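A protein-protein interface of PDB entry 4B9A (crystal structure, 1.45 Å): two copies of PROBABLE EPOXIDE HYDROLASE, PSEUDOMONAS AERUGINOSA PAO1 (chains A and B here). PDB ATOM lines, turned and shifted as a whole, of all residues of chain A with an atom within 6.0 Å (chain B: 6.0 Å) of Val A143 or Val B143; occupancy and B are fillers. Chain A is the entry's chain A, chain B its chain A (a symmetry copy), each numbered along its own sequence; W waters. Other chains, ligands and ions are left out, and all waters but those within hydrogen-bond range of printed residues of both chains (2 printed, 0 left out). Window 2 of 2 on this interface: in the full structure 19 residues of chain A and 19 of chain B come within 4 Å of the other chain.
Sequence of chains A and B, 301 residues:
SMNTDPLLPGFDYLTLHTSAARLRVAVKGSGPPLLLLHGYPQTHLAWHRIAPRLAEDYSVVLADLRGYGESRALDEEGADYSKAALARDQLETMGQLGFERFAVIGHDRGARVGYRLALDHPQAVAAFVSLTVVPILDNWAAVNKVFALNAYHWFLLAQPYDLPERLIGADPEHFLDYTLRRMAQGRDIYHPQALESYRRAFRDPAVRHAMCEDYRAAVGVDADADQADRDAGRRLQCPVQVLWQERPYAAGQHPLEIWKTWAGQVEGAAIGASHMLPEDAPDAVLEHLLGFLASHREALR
The backbone carbonyl oxygen of Val A143 sits close to the backbone carbonyl oxygen of Val B143 (3.4 Å).
The side-chain amide oxygen (OD1) of Asn B144 lies within hydrogen-bond range of the backbone NH (N) of Phe B147, 3.0 Å away.
The backbone NH (N) of Phe A147 lies within hydrogen-bond range of the side-chain amide oxygen (OD1) of Asn A144 (3.0 Å).
Trp A140 touches Lys B145.
C of Asn B144 touches CG1 of Val A143, 3.6 Å away.
N of Lys B145 touches CG1 of Val A143, at 3.8 Å.
CG1 of Val B143 touches C of Asn A144 (3.6 Å).
Trp B140 touches Lys A145.
Lys A145 touches Val B143 (N to CG1, 3.8 Å).
Ala A148 touches Ala B148 (CB to CB, 3.999 Å).
Phe B155 touches Ala A148 (CE1 to CB, 3.5 Å).
Phe A155 touches Ala B148.
Val A143 touches just these residues of chain B: Val B143, Asn B144 and Lys B145.
Of chain A, only Val A143 (3.4 Å), Asn A144 (3.6 Å) and Lys A145 (3.8 Å) come within 4 Å of Val B143.
Printed residues of chain B within 4 Å of Asn A144: Val B143.
Of the printed residues of chain B, Lys A145 touches Trp B140 and Val B143.
Printed residues of chain B within 4 Å of Trp A140: Lys B145.
Printed residues of chain A within 4 Å of Asn B144: Val A143.
Of the printed residues of chain A, Lys B145 touches Trp A140 and Val A143.
Ala B141 touches none of the printed residues of chain A.
Asp A138 touches none of the printed residues of chain B.
The nearest residue of chain A that does not touch Val B143 is Ala A148 (4.5 Å).
The nearest printed residue of chain B that does not touch Lys A145 is Phe B155 (4.02 Å).
Among the printed residues, 10 pairs touch across the chains.
Among the printed residues, no Asp or Glu carboxylate lies within 4 Å of a Lys or Arg side-chain nitrogen of the other chain.
Trp A140 touches Lys B145, and with the chains exchanged Lys A145 touches Trp B140.
Val B143 touches its own counterpart, Val A143.
Val A143 touches Asn B144, and with the chains exchanged Asn A144 touches Val B143.
Ala A148 touches its own counterpart, Ala B148.
Water W1 lies within hydrogen-bond range of O of Trp A140 (2.8 Å) and N of Lys B145 (2.9 Å).
Water W2 bridges O of Trp B140 (2.8 Å) and N of Lys A145 (2.9 Å).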
ATOM      1  N   ASP A 138       2.074  20.281 -18.723  1.00  0.00           N
ATOM      2  CA  ASP A 138       3.264  20.230 -19.552  1.00  0.00           C
ATOM      3  C   ASP A 138       4.246  21.303 -19.078  1.00  0.00           C
ATOM      4  O   ASP A 138       5.457  21.040 -19.021  1.00  0.00           O
ATOM      5  CB  ASP A 138       2.892  20.405 -21.023  1.00  0.00           C
ATOM      6  CG  ASP A 138       2.043  19.261 -21.531  1.00  0.00           C
ATOM      7  OD1 ASP A 138       2.655  18.271 -21.909  1.00  0.00           O
ATOM      8  OD2 ASP A 138       0.833  19.406 -21.539  1.00  0.00           O
ATOM      9  N   ASN A 139       3.778  22.513 -18.767  1.00  0.00           N
ATOM     10  CA  ASN A 139       4.669  23.536 -18.232  1.00  0.00           C
ATOM     11  C   ASN A 139       5.386  23.090 -16.970  1.00  0.00           C
ATOM     12  O   ASN A 139       6.617  23.224 -16.846  1.00  0.00           O
ATOM     13  CB  ASN A 139       3.970  24.854 -17.906  1.00  0.00           C
ATOM     14  CG  ASN A 139       3.324  25.561 -19.077  1.00  0.00           C
ATOM     15  OD1 ASN A 139       2.133  25.778 -19.044  1.00  0.00           O
ATOM     16  ND2 ASN A 139       4.062  25.938 -20.032  1.00  0.00           N
ATOM     17  N   TRP A 140       4.660  22.477 -16.046  1.00  0.00           N
ATOM     18  CA  TRP A 140       5.274  22.080 -14.790  1.00  0.00           C
ATOM     19  C   TRP A 140       6.328  21.009 -15.029  1.00  0.00           C
ATOM     20  O   TRP A 140       7.369  21.031 -14.370  1.00  0.00           O
ATOM     21  CB  TRP A 140       4.262  21.605 -13.735  1.00  0.00           C
ATOM     22  CG  TRP A 140       3.362  22.675 -13.194  1.00  0.00           C
ATOM     23  CD1 TRP A 140       2.006  22.567 -13.016  1.00  0.00           C
ATOM     24  CD2 TRP A 140       3.719  23.979 -12.703  1.00  0.00           C
ATOM     25  NE1 TRP A 140       1.522  23.682 -12.410  1.00  0.00           N
ATOM     26  CE2 TRP A 140       2.526  24.580 -12.235  1.00  0.00           C
ATOM     27  CE3 TRP A 140       4.938  24.681 -12.537  1.00  0.00           C
ATOM     28  CZ2 TRP A 140       2.492  25.882 -11.738  1.00  0.00           C
ATOM     29  CZ3 TRP A 140       4.892  25.964 -11.973  1.00  0.00           C
ATOM     30  CH2 TRP A 140       3.675  26.530 -11.566  1.00  0.00           C
ATOM     31  N   ALA A 141       6.093  20.116 -15.978  1.00  0.00           N
ATOM     32  CA  ALA A 141       7.066  19.066 -16.226  1.00  0.00           C
ATOM     33  C   ALA A 141       8.382  19.586 -16.800  1.00  0.00           C
ATOM     34  O   ALA A 141       9.421  18.890 -16.713  1.00  0.00           O
ATOM     35  CB  ALA A 141       6.469  18.029 -17.176  1.00  0.00           C
ATOM     36  N   ALA A 142       8.325  20.779 -17.395  1.00  0.00           N
ATOM     37  CA  ALA A 142       9.467  21.417 -18.015  1.00  0.00           C
ATOM     38  C   ALA A 142      10.269  22.335 -17.107  1.00  0.00           C
ATOM     39  O   ALA A 142      11.256  22.938 -17.552  1.00  0.00           O
ATOM     40  CB  ALA A 142       9.025  22.205 -19.243  1.00  0.00           C
ATOM     41  N   VAL A 143       9.908  22.430 -15.822  1.00  0.00           N
ATOM     42  CA  VAL A 143      10.615  23.358 -14.952  1.00  0.00           C
ATOM     43  C   VAL A 143      12.065  22.948 -14.797  1.00  0.00           C
ATOM     44  O   VAL A 143      12.383  21.825 -14.480  1.00  0.00           O
ATOM     45  CB  VAL A 143       9.913  23.491 -13.585  1.00  0.00           C
ATOM     46  CG1 VAL A 143      10.745  24.306 -12.632  1.00  0.00           C
ATOM     47  CG2 VAL A 143       8.541  24.072 -13.750  1.00  0.00           C
ATOM     48  N   ASN A 144      12.946  23.898 -14.992  1.00  0.00           N
ATOM     49  CA  ASN A 144      14.370  23.758 -14.745  1.00  0.00           C
ATOM     50  C   ASN A 144      14.884  25.177 -14.343  1.00  0.00           C
ATOM     51  O   ASN A 144      14.100  26.118 -14.205  1.00  0.00           O
ATOM     52  CB  ASN A 144      15.110  23.192 -15.952  1.00  0.00           C
ATOM     53  CG  ASN A 144      15.048  24.074 -17.198  1.00  0.00           C
ATOM     54  OD1 ASN A 144      14.642  25.224 -17.182  1.00  0.00           O
ATOM     55  ND2 ASN A 144      15.482  23.492 -18.307  1.00  0.00           N
ATOM     56  N   LYS A 145      16.205  25.274 -14.123  1.00  0.00           N
ATOM     57  CA  LYS A 145      16.826  26.497 -13.706  1.00  0.00           C
ATOM     58  C   LYS A 145      16.358  27.694 -14.530  1.00  0.00           C
ATOM     59  O   LYS A 145      15.876  28.707 -13.994  1.00  0.00           O
ATOM     60  CB  LYS A 145      18.324  26.338 -13.698  1.00  0.00           C
ATOM     61  CG  LYS A 145      19.077  27.608 -13.284  1.00  0.00           C
ATOM     62  CD  LYS A 145      20.561  27.553 -13.571  1.00  0.00           C
ATOM     63  CE  LYS A 145      21.323  28.730 -13.041  1.00  0.00           C
ATOM     64  NZ  LYS A 145      22.746  28.633 -13.433  1.00  0.00           N
ATOM     65  N   PHE A 147      13.926  28.082 -16.711  1.00  0.00           N
ATOM     66  CA  PHE A 147      12.475  28.323 -16.676  1.00  0.00           C
ATOM     67  C   PHE A 147      12.083  29.148 -15.438  1.00  0.00           C
ATOM     68  O   PHE A 147      11.343  30.127 -15.506  1.00  0.00           O
ATOM     69  CB  PHE A 147      11.685  27.028 -16.703  1.00  0.00           C
ATOM     70  CG  PHE A 147      10.193  27.236 -16.671  1.00  0.00           C
ATOM     71  CD1 PHE A 147       9.517  27.426 -15.508  1.00  0.00           C
ATOM     72  CD2 PHE A 147       9.475  27.310 -17.830  1.00  0.00           C
ATOM     73  CE1 PHE A 147       8.148  27.607 -15.495  1.00  0.00           C
ATOM     74  CE2 PHE A 147       8.114  27.553 -17.830  1.00  0.00           C
ATOM     75  CZ  PHE A 147       7.456  27.657 -16.647  1.00  0.00           C
ATOM     76  N   ALA A 148      12.595  28.714 -14.306  1.00  0.00           N
ATOM     77  CA  ALA A 148      12.230  29.335 -13.037  1.00  0.00           C
ATOM     78  C   ALA A 148      12.814  30.755 -12.909  1.00  0.00           C
ATOM     79  O   ALA A 148      12.199  31.596 -12.261  1.00  0.00           O
ATOM     80  CB  ALA A 148      12.568  28.425 -11.879  1.00  0.00           C
ATOM     81  N   PHE A 155       6.360  31.315  -9.498  1.00  0.00           N
ATOM     82  CA  PHE A 155       6.710  30.813  -8.173  1.00  0.00           C
ATOM     83  C   PHE A 155       6.414  31.806  -7.077  1.00  0.00           C
ATOM     84  O   PHE A 155       5.902  31.429  -6.028  1.00  0.00           O
ATOM     85  CB  PHE A 155       8.161  30.303  -8.209  1.00  0.00           C
ATOM     86  CG  PHE A 155       8.310  29.250  -9.289  1.00  0.00           C
ATOM     87  CD1 PHE A 155       7.879  27.937  -9.084  1.00  0.00           C
ATOM     88  CD2 PHE A 155       8.804  29.608 -10.552  1.00  0.00           C
ATOM     89  CE1 PHE A 155       7.912  27.003 -10.100  1.00  0.00           C
ATOM     90  CE2 PHE A 155       8.842  28.661 -11.580  1.00  0.00           C
ATOM     91  CZ  PHE A 155       8.369  27.358 -11.353  1.00  0.00           C
ATOM     92  N   ASP B 138      25.058  21.375  -8.160  1.00  0.00           N
ATOM     93  CA  ASP B 138      24.179  20.253  -7.887  1.00  0.00           C
ATOM     94  C   ASP B 138      22.772  20.782  -7.602  1.00  0.00           C
ATOM     95  O   ASP B 138      21.789  20.184  -8.067  1.00  0.00           O
ATOM     96  CB  ASP B 138      24.725  19.425  -6.726  1.00  0.00           C
ATOM     97  CG  ASP B 138      26.048  18.777  -7.066  1.00  0.00           C
ATOM     98  OD1 ASP B 138      25.981  17.710  -7.662  1.00  0.00           O
ATOM     99  OD2 ASP B 138      27.068  19.346  -6.719  1.00  0.00           O
ATOM    100  N   ASN B 139      22.633  21.861  -6.830  1.00  0.00           N
ATOM    101  CA  ASN B 139      21.316  22.445  -6.604  1.00  0.00           C
ATOM    102  C   ASN B 139      20.615  22.830  -7.894  1.00  0.00           C
ATOM    103  O   ASN B 139      19.439  22.490  -8.115  1.00  0.00           O
ATOM    104  CB  ASN B 139      21.335  23.688  -5.717  1.00  0.00           C
ATOM    105  CG  ASN B 139      21.849  23.480  -4.309  1.00  0.00           C
ATOM    106  OD1 ASN B 139      22.815  24.111  -3.941  1.00  0.00           O
ATOM    107  ND2 ASN B 139      21.222  22.685  -3.553  1.00  0.00           N
ATOM    108  N   TRP B 140      21.334  23.470  -8.805  1.00  0.00           N
ATOM    109  CA  TRP B 140      20.705  23.921 -10.036  1.00  0.00           C
ATOM    110  C   TRP B 140      20.251  22.731 -10.867  1.00  0.00           C
ATOM    111  O   TRP B 140      19.186  22.799 -11.484  1.00  0.00           O
ATOM    112  CB  TRP B 140      21.597  24.849 -10.876  1.00  0.00           C
ATOM    113  CG  TRP B 140      21.856  26.197 -10.273  1.00  0.00           C
ATOM    114  CD1 TRP B 140      23.075  26.824 -10.204  1.00  0.00           C
ATOM    115  CD2 TRP B 140      20.908  27.120  -9.709  1.00  0.00           C
ATOM    116  NE1 TRP B 140      22.932  28.073  -9.691  1.00  0.00           N
ATOM    117  CE2 TRP B 140      21.635  28.279  -9.343  1.00  0.00           C
ATOM    118  CE3 TRP B 140      19.502  27.124  -9.540  1.00  0.00           C
ATOM    119  CZ2 TRP B 140      21.035  29.365  -8.708  1.00  0.00           C
ATOM    120  CZ3 TRP B 140      18.908  28.255  -8.962  1.00  0.00           C
ATOM    121  CH2 TRP B 140      19.682  29.359  -8.577  1.00  0.00           C
ATOM    122  N   ALA B 141      21.010  21.646 -10.855  1.00  0.00           N
ATOM    123  CA  ALA B 141      20.622  20.494 -11.650  1.00  0.00           C
ATOM    124  C   ALA B 141      19.347  19.818 -11.150  1.00  0.00           C
ATOM    125  O   ALA B 141      18.689  19.077 -11.917  1.00  0.00           O
ATOM    126  CB  ALA B 141      21.763  19.478 -11.672  1.00  0.00           C
ATOM    127  N   ALA B 142      19.024  20.057  -9.877  1.00  0.00           N
ATOM    128  CA  ALA B 142      17.865  19.483  -9.227  1.00  0.00           C
ATOM    129  C   ALA B 142      16.598  20.318  -9.304  1.00  0.00           C
ATOM    130  O   ALA B 142      15.558  19.917  -8.764  1.00  0.00           O
ATOM    131  CB  ALA B 142      18.174  19.194  -7.762  1.00  0.00           C
ATOM    132  N   VAL B 143      16.632  21.458 -10.004  1.00  0.00           N
ATOM    133  CA  VAL B 143      15.452  22.311 -10.032  1.00  0.00           C
ATOM    134  C   VAL B 143      14.298  21.607 -10.713  1.00  0.00           C
ATOM    135  O   VAL B 143      14.413  21.096 -11.804  1.00  0.00           O
ATOM    136  CB  VAL B 143      15.759  23.670 -10.691  1.00  0.00           C
ATOM    137  CG1 VAL B 143      14.498  24.471 -10.880  1.00  0.00           C
ATOM    138  CG2 VAL B 143      16.775  24.429  -9.892  1.00  0.00           C
ATOM    139  N   ASN B 144      13.161  21.621 -10.062  1.00  0.00           N
ATOM    140  CA  ASN B 144      11.901  21.142 -10.603  1.00  0.00           C
ATOM    141  C   ASN B 144      10.784  21.998  -9.927  1.00  0.00           C
ATOM    142  O   ASN B 144      11.070  22.934  -9.177  1.00  0.00           O
ATOM    143  CB  ASN B 144      11.708  19.647 -10.371  1.00  0.00           C
ATOM    144  CG  ASN B 144      11.644  19.241  -8.900  1.00  0.00           C
ATOM    145  OD1 ASN B 144      11.531  20.046  -7.990  1.00  0.00           O
ATOM    146  ND2 ASN B 144      11.710  17.935  -8.685  1.00  0.00           N
ATOM    147  N   LYS B 145       9.524  21.671 -10.256  1.00  0.00           N
ATOM    148  CA  LYS B 145       8.389  22.388  -9.754  1.00  0.00           C
ATOM    149  C   LYS B 145       8.475  22.628  -8.249  1.00  0.00           C
ATOM    150  O   LYS B 145       8.386  23.770  -7.765  1.00  0.00           O
ATOM    151  CB  LYS B 145       7.117  21.693 -10.167  1.00  0.00           C
ATOM    152  CG  LYS B 145       5.845  22.380  -9.654  1.00  0.00           C
ATOM    153  CD  LYS B 145       4.601  21.531  -9.795  1.00  0.00           C
ATOM    154  CE  LYS B 145       3.336  22.248  -9.428  1.00  0.00           C
ATOM    155  NZ  LYS B 145       2.184  21.326  -9.518  1.00  0.00           N
ATOM    156  N   PHE B 147      10.907  22.241  -6.068  1.00  0.00           N
ATOM    157  CA  PHE B 147      12.095  22.993  -5.633  1.00  0.00           C
ATOM    158  C   PHE B 147      11.866  24.508  -5.763  1.00  0.00           C
ATOM    159  O   PHE B 147      12.137  25.295  -4.859  1.00  0.00           O
ATOM    160  CB  PHE B 147      13.335  22.591  -6.410  1.00  0.00           C
ATOM    161  CG  PHE B 147      14.573  23.339  -5.989  1.00  0.00           C
ATOM    162  CD1 PHE B 147      14.873  24.570  -6.479  1.00  0.00           C
ATOM    163  CD2 PHE B 147      15.408  22.825  -5.037  1.00  0.00           C
ATOM    164  CE1 PHE B 147      16.016  25.240  -6.089  1.00  0.00           C
ATOM    165  CE2 PHE B 147      16.521  23.516  -4.596  1.00  0.00           C
ATOM    166  CZ  PHE B 147      16.836  24.708  -5.165  1.00  0.00           C
ATOM    167  N   ALA B 148      11.368  24.890  -6.919  1.00  0.00           N
ATOM    168  CA  ALA B 148      11.193  26.307  -7.223  1.00  0.00           C
ATOM    169  C   ALA B 148      10.066  26.934  -6.382  1.00  0.00           C
ATOM    170  O   ALA B 148      10.143  28.119  -6.071  1.00  0.00           O
ATOM    171  CB  ALA B 148      11.040  26.520  -8.712  1.00  0.00           C
ATOM    172  N   PHE B 155      14.927  32.380  -6.949  1.00  0.00           N
ATOM    173  CA  PHE B 155      14.564  32.932  -8.250  1.00  0.00           C
ATOM    174  C   PHE B 155      14.208  34.396  -8.183  1.00  0.00           C
ATOM    175  O   PHE B 155      14.615  35.169  -9.044  1.00  0.00           O
ATOM    176  CB  PHE B 155      13.486  32.033  -8.881  1.00  0.00           C
ATOM    177  CG  PHE B 155      13.994  30.609  -8.975  1.00  0.00           C
ATOM    178  CD1 PHE B 155      14.876  30.219  -9.985  1.00  0.00           C
ATOM    179  CD2 PHE B 155      13.652  29.678  -7.983  1.00  0.00           C
ATOM    180  CE1 PHE B 155      15.426  28.954 -10.011  1.00  0.00           C
ATOM    181  CE2 PHE B 155      14.205  28.394  -8.011  1.00  0.00           C
ATOM    182  CZ  PHE B 155      15.117  28.044  -9.021  1.00  0.00           C
HETATM  183  O   HOH W   1       9.006  19.813 -12.463  1.00  0.00           O
HETATM  184  O   HOH W   2      17.856  22.859 -13.939  1.00  0.00           O
